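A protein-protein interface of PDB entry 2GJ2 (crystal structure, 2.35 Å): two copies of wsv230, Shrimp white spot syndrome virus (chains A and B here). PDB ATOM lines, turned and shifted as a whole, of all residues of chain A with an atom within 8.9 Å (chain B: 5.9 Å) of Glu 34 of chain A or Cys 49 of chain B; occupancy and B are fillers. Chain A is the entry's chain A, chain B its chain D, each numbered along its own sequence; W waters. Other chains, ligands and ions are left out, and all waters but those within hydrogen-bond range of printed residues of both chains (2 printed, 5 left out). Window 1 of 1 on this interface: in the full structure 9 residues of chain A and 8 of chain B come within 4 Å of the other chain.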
ATOM      1  N   ASP A  12      18.586 -34.989   6.693  1.00  0.00           N
ATOM      2  CA  ASP A  12      19.349 -33.759   6.567  1.00  0.00           C
ATOM      3  C   ASP A  12      20.220 -33.959   5.361  1.00  0.00           C
ATOM      4  O   ASP A  12      20.427 -35.086   4.933  1.00  0.00           O
ATOM      5  CB  ASP A  12      20.266 -33.547   7.778  1.00  0.00           C
ATOM      6  CG  ASP A  12      19.498 -33.366   9.064  1.00  0.00           C
ATOM      7  OD1 ASP A  12      18.275 -33.110   8.985  1.00  0.00           O
ATOM      8  OD2 ASP A  12      20.129 -33.468  10.148  1.00  0.00           O
ATOM      9  N   PHE A  13      20.761 -32.879   4.827  1.00  0.00           N
ATOM     10  CA  PHE A  13      21.625 -33.023   3.690  1.00  0.00           C
ATOM     11  C   PHE A  13      22.735 -31.985   3.644  1.00  0.00           C
ATOM     12  O   PHE A  13      22.666 -30.949   4.295  1.00  0.00           O
ATOM     13  CB  PHE A  13      20.793 -33.040   2.390  1.00  0.00           C
ATOM     14  CG  PHE A  13      19.801 -31.914   2.255  1.00  0.00           C
ATOM     15  CD1 PHE A  13      20.130 -30.759   1.533  1.00  0.00           C
ATOM     16  CD2 PHE A  13      18.514 -32.034   2.776  1.00  0.00           C
ATOM     17  CE1 PHE A  13      19.185 -29.738   1.322  1.00  0.00           C
ATOM     18  CE2 PHE A  13      17.571 -31.032   2.575  1.00  0.00           C
ATOM     19  CZ  PHE A  13      17.915 -29.866   1.836  1.00  0.00           C
ATOM     20  N   MET A  27      17.766 -21.473   1.522  1.00  0.00           N
ATOM     21  CA  MET A  27      17.287 -22.645   2.242  1.00  0.00           C
ATOM     22  C   MET A  27      16.266 -22.277   3.298  1.00  0.00           C
ATOM     23  O   MET A  27      15.322 -23.028   3.532  1.00  0.00           O
ATOM     24  CB  MET A  27      18.439 -23.421   2.864  1.00  0.00           C
ATOM     25  CG  MET A  27      19.298 -24.109   1.830  1.00  0.00           C
ATOM     26  SD  MET A  27      18.357 -25.022   0.564  1.00  0.00           S
ATOM     27  CE  MET A  27      17.309 -26.048   1.559  1.00  0.00           C
ATOM     28  N   LYS A  28      16.416 -21.103   3.900  1.00  0.00           N
ATOM     29  CA  LYS A  28      15.468 -20.675   4.927  1.00  0.00           C
ATOM     30  C   LYS A  28      14.082 -20.272   4.407  1.00  0.00           C
ATOM     31  O   LYS A  28      13.252 -19.800   5.169  1.00  0.00           O
ATOM     32  CB  LYS A  28      16.068 -19.543   5.762  1.00  0.00           C
ATOM     33  CG  LYS A  28      16.905 -20.062   6.917  1.00  0.00           C
ATOM     34  CD  LYS A  28      18.227 -19.321   7.039  1.00  0.00           C
ATOM     35  CE  LYS A  28      18.023 -17.846   7.300  1.00  0.00           C
ATOM     36  NZ  LYS A  28      19.340 -17.172   7.447  1.00  0.00           N
ATOM     37  N   PHE A  30      12.309 -22.527   2.784  1.00  0.00           N
ATOM     38  CA  PHE A  30      11.565 -23.771   2.719  1.00  0.00           C
ATOM     39  C   PHE A  30      10.974 -24.028   4.099  1.00  0.00           C
ATOM     40  O   PHE A  30      11.632 -23.823   5.121  1.00  0.00           O
ATOM     41  CB  PHE A  30      12.464 -24.932   2.284  1.00  0.00           C
ATOM     42  CG  PHE A  30      12.872 -24.877   0.829  1.00  0.00           C
ATOM     43  CD1 PHE A  30      13.999 -24.163   0.429  1.00  0.00           C
ATOM     44  CD2 PHE A  30      12.137 -25.557  -0.137  1.00  0.00           C
ATOM     45  CE1 PHE A  30      14.387 -24.135  -0.913  1.00  0.00           C
ATOM     46  CE2 PHE A  30      12.514 -25.532  -1.474  1.00  0.00           C
ATOM     47  CZ  PHE A  30      13.642 -24.820  -1.862  1.00  0.00           C
ATOM     48  N   ASP A  31       9.723 -24.459   4.129  1.00  0.00           N
ATOM     49  CA  ASP A  31       9.045 -24.709   5.390  1.00  0.00           C
ATOM     50  C   ASP A  31       9.463 -26.038   6.035  1.00  0.00           C
ATOM     51  O   ASP A  31       8.991 -26.373   7.126  1.00  0.00           O
ATOM     52  CB  ASP A  31       7.517 -24.673   5.181  1.00  0.00           C
ATOM     53  CG  ASP A  31       6.982 -23.259   4.912  1.00  0.00           C
ATOM     54  OD1 ASP A  31       7.621 -22.500   4.151  1.00  0.00           O
ATOM     55  OD2 ASP A  31       5.907 -22.912   5.452  1.00  0.00           O
ATOM     56  N   THR A  32      10.339 -26.794   5.368  1.00  0.00           N
ATOM     57  CA  THR A  32      10.798 -28.068   5.922  1.00  0.00           C
ATOM     58  C   THR A  32      12.179 -27.972   6.580  1.00  0.00           C
ATOM     59  O   THR A  32      12.629 -28.914   7.221  1.00  0.00           O
ATOM     60  CB  THR A  32      10.862 -29.171   4.835  1.00  0.00           C
ATOM     61  OG1 THR A  32      11.455 -28.633   3.651  1.00  0.00           O
ATOM     62  CG2 THR A  32       9.471 -29.720   4.524  1.00  0.00           C
ATOM     63  N   VAL A  33      12.841 -26.834   6.425  1.00  0.00           N
ATOM     64  CA  VAL A  33      14.174 -26.635   6.982  1.00  0.00           C
ATOM     65  C   VAL A  33      14.113 -26.109   8.407  1.00  0.00           C
ATOM     66  O   VAL A  33      13.522 -25.070   8.656  1.00  0.00           O
ATOM     67  CB  VAL A  33      14.978 -25.656   6.089  1.00  0.00           C
ATOM     68  CG1 VAL A  33      16.375 -25.422   6.660  1.00  0.00           C
ATOM     69  CG2 VAL A  33      15.081 -26.243   4.653  1.00  0.00           C
ATOM     70  N   GLU A  34      14.712 -26.848   9.340  1.00  0.00           N
ATOM     71  CA  GLU A  34      14.746 -26.476  10.755  1.00  0.00           C
ATOM     72  C   GLU A  34      15.869 -25.488  10.901  1.00  0.00           C
ATOM     73  O   GLU A  34      15.702 -24.442  11.490  1.00  0.00           O
ATOM     74  CB  GLU A  34      15.054 -27.696  11.624  1.00  0.00           C
ATOM     75  CG  GLU A  34      15.070 -27.478  13.168  1.00  0.00           C
ATOM     76  CD  GLU A  34      15.701 -28.674  13.915  1.00  0.00           C
ATOM     77  OE1 GLU A  34      16.972 -28.808  13.848  1.00  0.00           O
ATOM     78  OE2 GLU A  34      14.931 -29.474  14.542  1.00  0.00           O
ATOM     79  N   ALA A  35      17.016 -25.830  10.328  1.00  0.00           N
ATOM     80  CA  ALA A  35      18.201 -24.990  10.397  1.00  0.00           C
ATOM     81  C   ALA A  35      19.167 -25.247   9.236  1.00  0.00           C
ATOM     82  O   ALA A  35      19.153 -26.303   8.599  1.00  0.00           O
ATOM     83  CB  ALA A  35      18.941 -25.224  11.756  1.00  0.00           C
ATOM     84  N   VAL A  36      20.015 -24.259   8.990  1.00  0.00           N
ATOM     85  CA  VAL A  36      21.032 -24.315   7.957  1.00  0.00           C
ATOM     86  C   VAL A  36      22.296 -23.870   8.658  1.00  0.00           C
ATOM     87  O   VAL A  36      22.323 -22.789   9.222  1.00  0.00           O
ATOM     88  CB  VAL A  36      20.726 -23.331   6.810  1.00  0.00           C
ATOM     89  CG1 VAL A  36      21.901 -23.294   5.813  1.00  0.00           C
ATOM     90  CG2 VAL A  36      19.461 -23.747   6.124  1.00  0.00           C
ATOM     91  N   ARG A  37      23.335 -24.694   8.643  1.00  0.00           N
ATOM     92  CA  ARG A  37      24.582 -24.325   9.317  1.00  0.00           C
ATOM     93  C   ARG A  37      25.705 -24.360   8.306  1.00  0.00           C
ATOM     94  O   ARG A  37      25.685 -25.168   7.402  1.00  0.00           O
ATOM     95  CB  ARG A  37      24.891 -25.301  10.459  1.00  0.00           C
ATOM     96  CG  ARG A  37      23.824 -25.357  11.539  1.00  0.00           C
ATOM     97  CD  ARG A  37      23.976 -26.580  12.445  1.00  0.00           C
ATOM     98  NE  ARG A  37      24.870 -26.373  13.584  1.00  0.00           N
ATOM     99  CZ  ARG A  37      24.713 -25.424  14.508  1.00  0.00           C
ATOM    100  NH1 ARG A  37      23.696 -24.573  14.437  1.00  0.00           N
ATOM    101  NH2 ARG A  37      25.567 -25.338  15.520  1.00  0.00           N
ATOM    102  N   MET A  47      25.296 -27.493   6.023  1.00  0.00           N
ATOM    103  CA  MET A  47      24.489 -28.600   6.493  1.00  0.00           C
ATOM    104  C   MET A  47      23.086 -28.031   6.576  1.00  0.00           C
ATOM    105  O   MET A  47      22.903 -26.900   7.020  1.00  0.00           O
ATOM    106  CB  MET A  47      24.964 -29.093   7.874  1.00  0.00           C
ATOM    107  N   VAL A  48      22.112 -28.796   6.102  1.00  0.00           N
ATOM    108  CA  VAL A  48      20.727 -28.381   6.139  1.00  0.00           C
ATOM    109  C   VAL A  48      19.986 -29.447   6.956  1.00  0.00           C
ATOM    110  O   VAL A  48      20.016 -30.631   6.609  1.00  0.00           O
ATOM    111  CB  VAL A  48      20.102 -28.344   4.741  1.00  0.00           C
ATOM    112  CG1 VAL A  48      18.750 -27.743   4.842  1.00  0.00           C
ATOM    113  CG2 VAL A  48      20.984 -27.551   3.751  1.00  0.00           C
ATOM    114  N   CYS A  49      19.340 -29.022   8.044  1.00  0.00           N
ATOM    115  CA  CYS A  49      18.570 -29.905   8.936  1.00  0.00           C
ATOM    116  C   CYS A  49      17.076 -29.906   8.582  1.00  0.00           C
ATOM    117  O   CYS A  49      16.450 -28.871   8.502  1.00  0.00           O
ATOM    118  CB  CYS A  49      18.740 -29.440  10.405  1.00  0.00           C
ATOM    119  SG  CYS A  49      17.732 -30.367  11.609  1.00  0.00           S
ATOM    120  N   LEU A  50      16.495 -31.067   8.367  1.00  0.00           N
ATOM    121  CA  LEU A  50      15.074 -31.119   8.064  1.00  0.00           C
ATOM    122  C   LEU A  50      14.273 -31.268   9.357  1.00  0.00           C
ATOM    123  O   LEU A  50      14.690 -32.012  10.245  1.00  0.00           O
ATOM    124  CB  LEU A  50      14.765 -32.308   7.154  1.00  0.00           C
ATOM    125  CG  LEU A  50      14.921 -32.054   5.662  1.00  0.00           C
ATOM    126  CD1 LEU A  50      14.252 -33.173   4.884  1.00  0.00           C
ATOM    127  CD2 LEU A  50      14.276 -30.715   5.312  1.00  0.00           C
ATOM    128  N   LYS A  51      13.134 -30.574   9.458  1.00  0.00           N
ATOM    129  CA  LYS A  51      12.269 -30.660  10.635  1.00  0.00           C
ATOM    130  C   LYS A  51      11.847 -32.111  10.799  1.00  0.00           C
ATOM    131  O   LYS A  51      11.669 -32.817   9.814  1.00  0.00           O
ATOM    132  CB  LYS A  51      11.003 -29.815  10.468  1.00  0.00           C
ATOM    133  CG  LYS A  51      11.222 -28.316  10.330  1.00  0.00           C
ATOM    134  CD  LYS A  51       9.885 -27.589  10.461  1.00  0.00           C
ATOM    135  CE  LYS A  51       9.901 -26.169   9.892  1.00  0.00           C
ATOM    136  NZ  LYS A  51      10.772 -25.203  10.616  1.00  0.00           N
ATOM    137  N   GLN A  52      11.684 -32.557  12.042  1.00  0.00           N
ATOM    138  CA  GLN A  52      11.291 -33.931  12.305  1.00  0.00           C
ATOM    139  C   GLN A  52      10.013 -34.235  11.544  1.00  0.00           C
ATOM    140  O   GLN A  52       9.103 -33.415  11.507  1.00  0.00           O
ATOM    141  CB  GLN A  52      11.092 -34.138  13.807  1.00  0.00           C
ATOM    142  CG  GLN A  52      10.718 -35.562  14.207  1.00  0.00           C
ATOM    143  CD  GLN A  52      10.785 -35.805  15.722  1.00  0.00           C
ATOM    144  OE1 GLN A  52      11.871 -35.951  16.306  1.00  0.00           O
ATOM    145  NE2 GLN A  52       9.623 -35.837  16.360  1.00  0.00           N
ATOM    146  N   GLY A  53       9.962 -35.400  10.908  1.00  0.00           N
ATOM    147  CA  GLY A  53       8.772 -35.798  10.167  1.00  0.00           C
ATOM    148  C   GLY A  53       8.524 -35.139   8.818  1.00  0.00           C
ATOM    149  O   GLY A  53       7.523 -35.426   8.152  1.00  0.00           O
ATOM    150  N   SER A  54       9.439 -34.268   8.403  1.00  0.00           N
ATOM    151  CA  SER A  54       9.307 -33.554   7.140  1.00  0.00           C
ATOM    152  C   SER A  54      10.076 -34.149   5.976  1.00  0.00           C
ATOM    153  O   SER A  54      11.071 -34.856   6.151  1.00  0.00           O
ATOM    154  CB  SER A  54       9.750 -32.117   7.320  1.00  0.00           C
ATOM    155  OG  SER A  54       8.919 -31.473   8.259  1.00  0.00           O
ATOM    156  N   PHE A  56      11.862 -32.992   2.320  1.00  0.00           N
ATOM    157  CA  PHE A  56      12.316 -31.870   1.507  1.00  0.00           C
ATOM    158  C   PHE A  56      12.102 -32.233   0.038  1.00  0.00           C
ATOM    159  O   PHE A  56      12.616 -33.256  -0.425  1.00  0.00           O
ATOM    160  CB  PHE A  56      13.790 -31.593   1.742  1.00  0.00           C
ATOM    161  CG  PHE A  56      14.326 -30.493   0.893  1.00  0.00           C
ATOM    162  CD1 PHE A  56      14.088 -29.163   1.232  1.00  0.00           C
ATOM    163  CD2 PHE A  56      15.033 -30.785  -0.284  1.00  0.00           C
ATOM    164  CE1 PHE A  56      14.543 -28.127   0.413  1.00  0.00           C
ATOM    165  CE2 PHE A  56      15.498 -29.762  -1.115  1.00  0.00           C
ATOM    166  CZ  PHE A  56      15.252 -28.426  -0.770  1.00  0.00           C
ATOM    167  N   ASP B  12      12.947 -33.071  19.766  1.00  0.00           N
ATOM    168  CA  ASP B  12      13.719 -31.916  20.134  1.00  0.00           C
ATOM    169  C   ASP B  12      13.119 -31.421  21.448  1.00  0.00           C
ATOM    170  O   ASP B  12      12.017 -31.831  21.828  1.00  0.00           O
ATOM    171  CB  ASP B  12      13.514 -30.843  19.083  1.00  0.00           C
ATOM    172  CG  ASP B  12      14.336 -31.078  17.878  1.00  0.00           C
ATOM    173  OD1 ASP B  12      15.045 -32.096  17.857  1.00  0.00           O
ATOM    174  OD2 ASP B  12      14.297 -30.234  16.966  1.00  0.00           O
ATOM    175  N   PHE B  13      13.819 -30.531  22.140  1.00  0.00           N
ATOM    176  CA  PHE B  13      13.252 -30.029  23.356  1.00  0.00           C
ATOM    177  C   PHE B  13      13.927 -28.789  23.794  1.00  0.00           C
ATOM    178  O   PHE B  13      15.055 -28.514  23.395  1.00  0.00           O
ATOM    179  CB  PHE B  13      13.279 -31.095  24.451  1.00  0.00           C
ATOM    180  CG  PHE B  13      14.644 -31.650  24.734  1.00  0.00           C
ATOM    181  CD1 PHE B  13      15.498 -31.017  25.644  1.00  0.00           C
ATOM    182  CD2 PHE B  13      15.047 -32.843  24.145  1.00  0.00           C
ATOM    183  CE1 PHE B  13      16.705 -31.562  25.970  1.00  0.00           C
ATOM    184  CE2 PHE B  13      16.264 -33.399  24.462  1.00  0.00           C
ATOM    185  CZ  PHE B  13      17.093 -32.765  25.371  1.00  0.00           C
ATOM    186  N   THR B  32      23.264 -38.276  21.150  1.00  0.00           N
ATOM    187  CA  THR B  32      21.974 -38.071  20.482  1.00  0.00           C
ATOM    188  C   THR B  32      21.659 -36.639  20.060  1.00  0.00           C
ATOM    189  O   THR B  32      20.648 -36.398  19.414  1.00  0.00           O
ATOM    190  CB  THR B  32      20.823 -38.540  21.397  1.00  0.00           C
ATOM    191  OG1 THR B  32      20.948 -37.902  22.686  1.00  0.00           O
ATOM    192  CG2 THR B  32      20.858 -40.066  21.577  1.00  0.00           C
ATOM    193  N   VAL B  33      22.517 -35.693  20.413  1.00  0.00           N
ATOM    194  CA  VAL B  33      22.265 -34.299  20.084  1.00  0.00           C
ATOM    195  C   VAL B  33      22.959 -33.773  18.832  1.00  0.00           C
ATOM    196  O   VAL B  33      24.186 -33.696  18.781  1.00  0.00           O
ATOM    197  CB  VAL B  33      22.654 -33.363  21.274  1.00  0.00           C
ATOM    198  CG1 VAL B  33      22.618 -31.920  20.825  1.00  0.00           C
ATOM    199  CG2 VAL B  33      21.709 -33.553  22.435  1.00  0.00           C
ATOM    200  N   GLU B  34      22.164 -33.400  17.833  1.00  0.00           N
ATOM    201  CA  GLU B  34      22.669 -32.844  16.580  1.00  0.00           C
ATOM    202  C   GLU B  34      23.204 -31.466  16.954  1.00  0.00           C
ATOM    203  O   GLU B  34      24.369 -31.170  16.722  1.00  0.00           O
ATOM    204  CB  GLU B  34      21.522 -32.717  15.559  1.00  0.00           C
ATOM    205  CG  GLU B  34      21.881 -32.473  14.073  1.00  0.00           C
ATOM    206  CD  GLU B  34      20.690 -31.903  13.253  1.00  0.00           C
ATOM    207  OE1 GLU B  34      20.256 -30.737  13.536  1.00  0.00           O
ATOM    208  OE2 GLU B  34      20.191 -32.611  12.336  1.00  0.00           O
ATOM    209  N   ALA B  35      22.364 -30.636  17.568  1.00  0.00           N
ATOM    210  CA  ALA B  35      22.794 -29.281  17.960  1.00  0.00           C
ATOM    211  C   ALA B  35      22.042 -28.634  19.130  1.00  0.00           C
ATOM    212  O   ALA B  35      21.002 -29.113  19.577  1.00  0.00           O
ATOM    213  CB  ALA B  35      22.728 -28.348  16.752  1.00  0.00           C
ATOM    214  N   VAL B  36      22.577 -27.515  19.599  1.00  0.00           N
ATOM    215  CA  VAL B  36      21.994 -26.781  20.704  1.00  0.00           C
ATOM    216  C   VAL B  36      22.006 -25.307  20.318  1.00  0.00           C
ATOM    217  O   VAL B  36      23.025 -24.781  19.884  1.00  0.00           O
ATOM    218  CB  VAL B  36      22.819 -27.012  21.991  1.00  0.00           C
ATOM    219  CG1 VAL B  36      22.294 -26.162  23.118  1.00  0.00           C
ATOM    220  CG2 VAL B  36      22.752 -28.459  22.387  1.00  0.00           C
ATOM    221  N   MET B  47      17.351 -24.570  22.745  1.00  0.00           N
ATOM    222  CA  MET B  47      16.639 -25.594  22.010  1.00  0.00           C
ATOM    223  C   MET B  47      17.626 -26.750  21.831  1.00  0.00           C
ATOM    224  O   MET B  47      18.777 -26.534  21.501  1.00  0.00           O
ATOM    225  CB  MET B  47      16.159 -25.060  20.653  1.00  0.00           C
ATOM    226  N   VAL B  48      17.208 -27.975  22.103  1.00  0.00           N
ATOM    227  CA  VAL B  48      18.108 -29.084  21.907  1.00  0.00           C
ATOM    228  C   VAL B  48      17.550 -29.902  20.763  1.00  0.00           C
ATOM    229  O   VAL B  48      16.468 -30.473  20.903  1.00  0.00           O
ATOM    230  CB  VAL B  48      18.188 -29.984  23.144  1.00  0.00           C
ATOM    231  CG1 VAL B  48      18.848 -31.308  22.786  1.00  0.00           C
ATOM    232  CG2 VAL B  48      18.969 -29.268  24.268  1.00  0.00           C
ATOM    233  N   CYS B  49      18.264 -29.961  19.632  1.00  0.00           N
ATOM    234  CA  CYS B  49      17.772 -30.750  18.500  1.00  0.00           C
ATOM    235  C   CYS B  49      18.370 -32.111  18.638  1.00  0.00           C
ATOM    236  O   CYS B  49      19.534 -32.234  18.958  1.00  0.00           O
ATOM    237  CB  CYS B  49      18.068 -30.036  17.180  1.00  0.00           C
ATOM    238  SG  CYS B  49      17.569 -30.964  15.694  1.00  0.00           S
ATOM    239  N   LEU B  50      17.588 -33.137  18.371  1.00  0.00           N
ATOM    240  CA  LEU B  50      18.098 -34.488  18.499  1.00  0.00           C
ATOM    241  C   LEU B  50      18.355 -35.151  17.138  1.00  0.00           C
ATOM    242  O   LEU B  50      17.691 -34.839  16.167  1.00  0.00           O
ATOM    243  CB  LEU B  50      17.091 -35.330  19.297  1.00  0.00           C
ATOM    244  CG  LEU B  50      16.846 -35.023  20.781  1.00  0.00           C
ATOM    245  CD1 LEU B  50      15.984 -36.161  21.354  1.00  0.00           C
ATOM    246  CD2 LEU B  50      18.171 -34.917  21.573  1.00  0.00           C
ATOM    247  N   LYS B  51      19.310 -36.074  17.072  1.00  0.00           N
ATOM    248  CA  LYS B  51      19.592 -36.775  15.813  1.00  0.00           C
ATOM    249  C   LYS B  51      18.301 -37.436  15.338  1.00  0.00           C
ATOM    250  O   LYS B  51      17.450 -37.776  16.144  1.00  0.00           O
ATOM    251  CB  LYS B  51      20.692 -37.833  16.013  1.00  0.00           C
ATOM    252  CG  LYS B  51      22.111 -37.249  16.156  1.00  0.00           C
ATOM    253  CD  LYS B  51      23.116 -38.340  16.458  1.00  0.00           C
ATOM    254  CE  LYS B  51      24.547 -37.936  16.093  1.00  0.00           C
ATOM    255  NZ  LYS B  51      25.228 -36.949  16.985  1.00  0.00           N
HETATM  256  O   HOH W   1      25.633 -28.451  15.208  1.00  0.00           O
HETATM  257  O   HOH W   2      14.867 -37.154  17.011  1.00  0.00           O
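The side-chain carboxylate (OE2) of Glu 34 of chain B sits close to the side-chain carboxylate (OD2) of Asp 12 of chain A, at 2.4 Å. The side-chain carboxylate (OE1) of Glu 34 of chain B sits close to the side-chain sulfur (SG) of Cys 49 of chain A (3.2 Å). OE2 of Glu 34 of chain A lies close to OD2 of Asp 12 of chain B, 2.6 Å away. The side-chain sulfur (SG) of Cys 49 of chain B sits close to the side-chain carboxylate (OE1) of Glu 34 of chain A, at 2.9 Å.
Glu 34 of chain A touches Glu 34 of chain B.
The side-chain carboxylate of Asp 12 of chain A lies close to the backbone NH of Leu 50 of chain A (2.8 Å). N of Cys 49 of chain B is in hydrogen-bond range of O of Ala 35 of chain B. The backbone NH (N) of Cys 49 of chain A lies within hydrogen-bond range of the backbone carbonyl oxygen (O) of Ala 35 of chain A (2.8 Å). The side-chain carboxylate (OD1) of Asp 12 of chain B is in hydrogen-bond range of the backbone NH (N) of Leu 50 of chain B (2.8 Å).
Water W1 lies within hydrogen-bond range of NE of Arg 37 of chain A (2.7 Å) and O of Glu 34 of chain B (3.4 Å). Water W2 lies within hydrogen-bond range of O of Lys 51 of chain B (2.8 Å) and OE1 of Gln 52 of chain A (3.3 Å).
Asp 12 of chain A touches Glu 34 of chain B, and with the chains exchanged Glu 34 of chain A touches Asp 12 of chain B. Glu 34 of chain B touches its own counterpart, Glu 34 of chain A. Glu 34 of chain A touches Cys 49 of chain B, and with the chains exchanged Cys 49 of chain A touches Glu 34 of chain B. Positions printed for both chains: 12, 13, 32, 33, 34, 35, 36, 47, 48, 49, 50 and 51.
Printed residues of chain B that touch a printed residue of chain A: Asp 12, Glu 34 and Cys 49. Along chain B the printed residues that touch a printed residue of chain A span positions 12 to 49. Of the 21 printed residues of chain A, 3 touch a printed residue of chain B. Printed residues of chain A that touch a printed residue of chain B: Asp 12, Glu 34 and Cys 49. Among the printed residues, no Asp or Glu carboxylate lies within 4 Å of a Lys or Arg side-chain nitrogen of the other chain.
Printed residues of chain B within 4 Å of Asp 12 of chain A: Glu 34 (2.4 Å). Glu 34 of chain A touches just these residues of chain B: Asp 12 (2.6 Å), Glu 34 (3.8 Å) and Cys 49 (2.9 Å). Printed residues of chain B within 4 Å of Cys 49 of chain A: Glu 34 (3.2 Å). Leu 50 of chain A touches none of the printed residues of chain B. Lys 51 of chain A touches none of the printed residues of chain B. Printed residues of chain A within 4 Å of Asp 12 of chain B: Glu 34. Printed residues of chain A within 4 Å of Glu 34 of chain B: Asp 12, Glu 34 and Cys 49. No residue of chain A comes within 4 Å of Val 48 of chain B. Cys 49 of chain B touches one residue of chain A. The nearest printed residue of chain B that does not touch Glu 34 of chain A is Leu 50 of chain B (5.9 Å). The nearest printed residue of chain A that does not touch Glu 34 of chain B is Leu 50 of chain A (5.6 Å).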
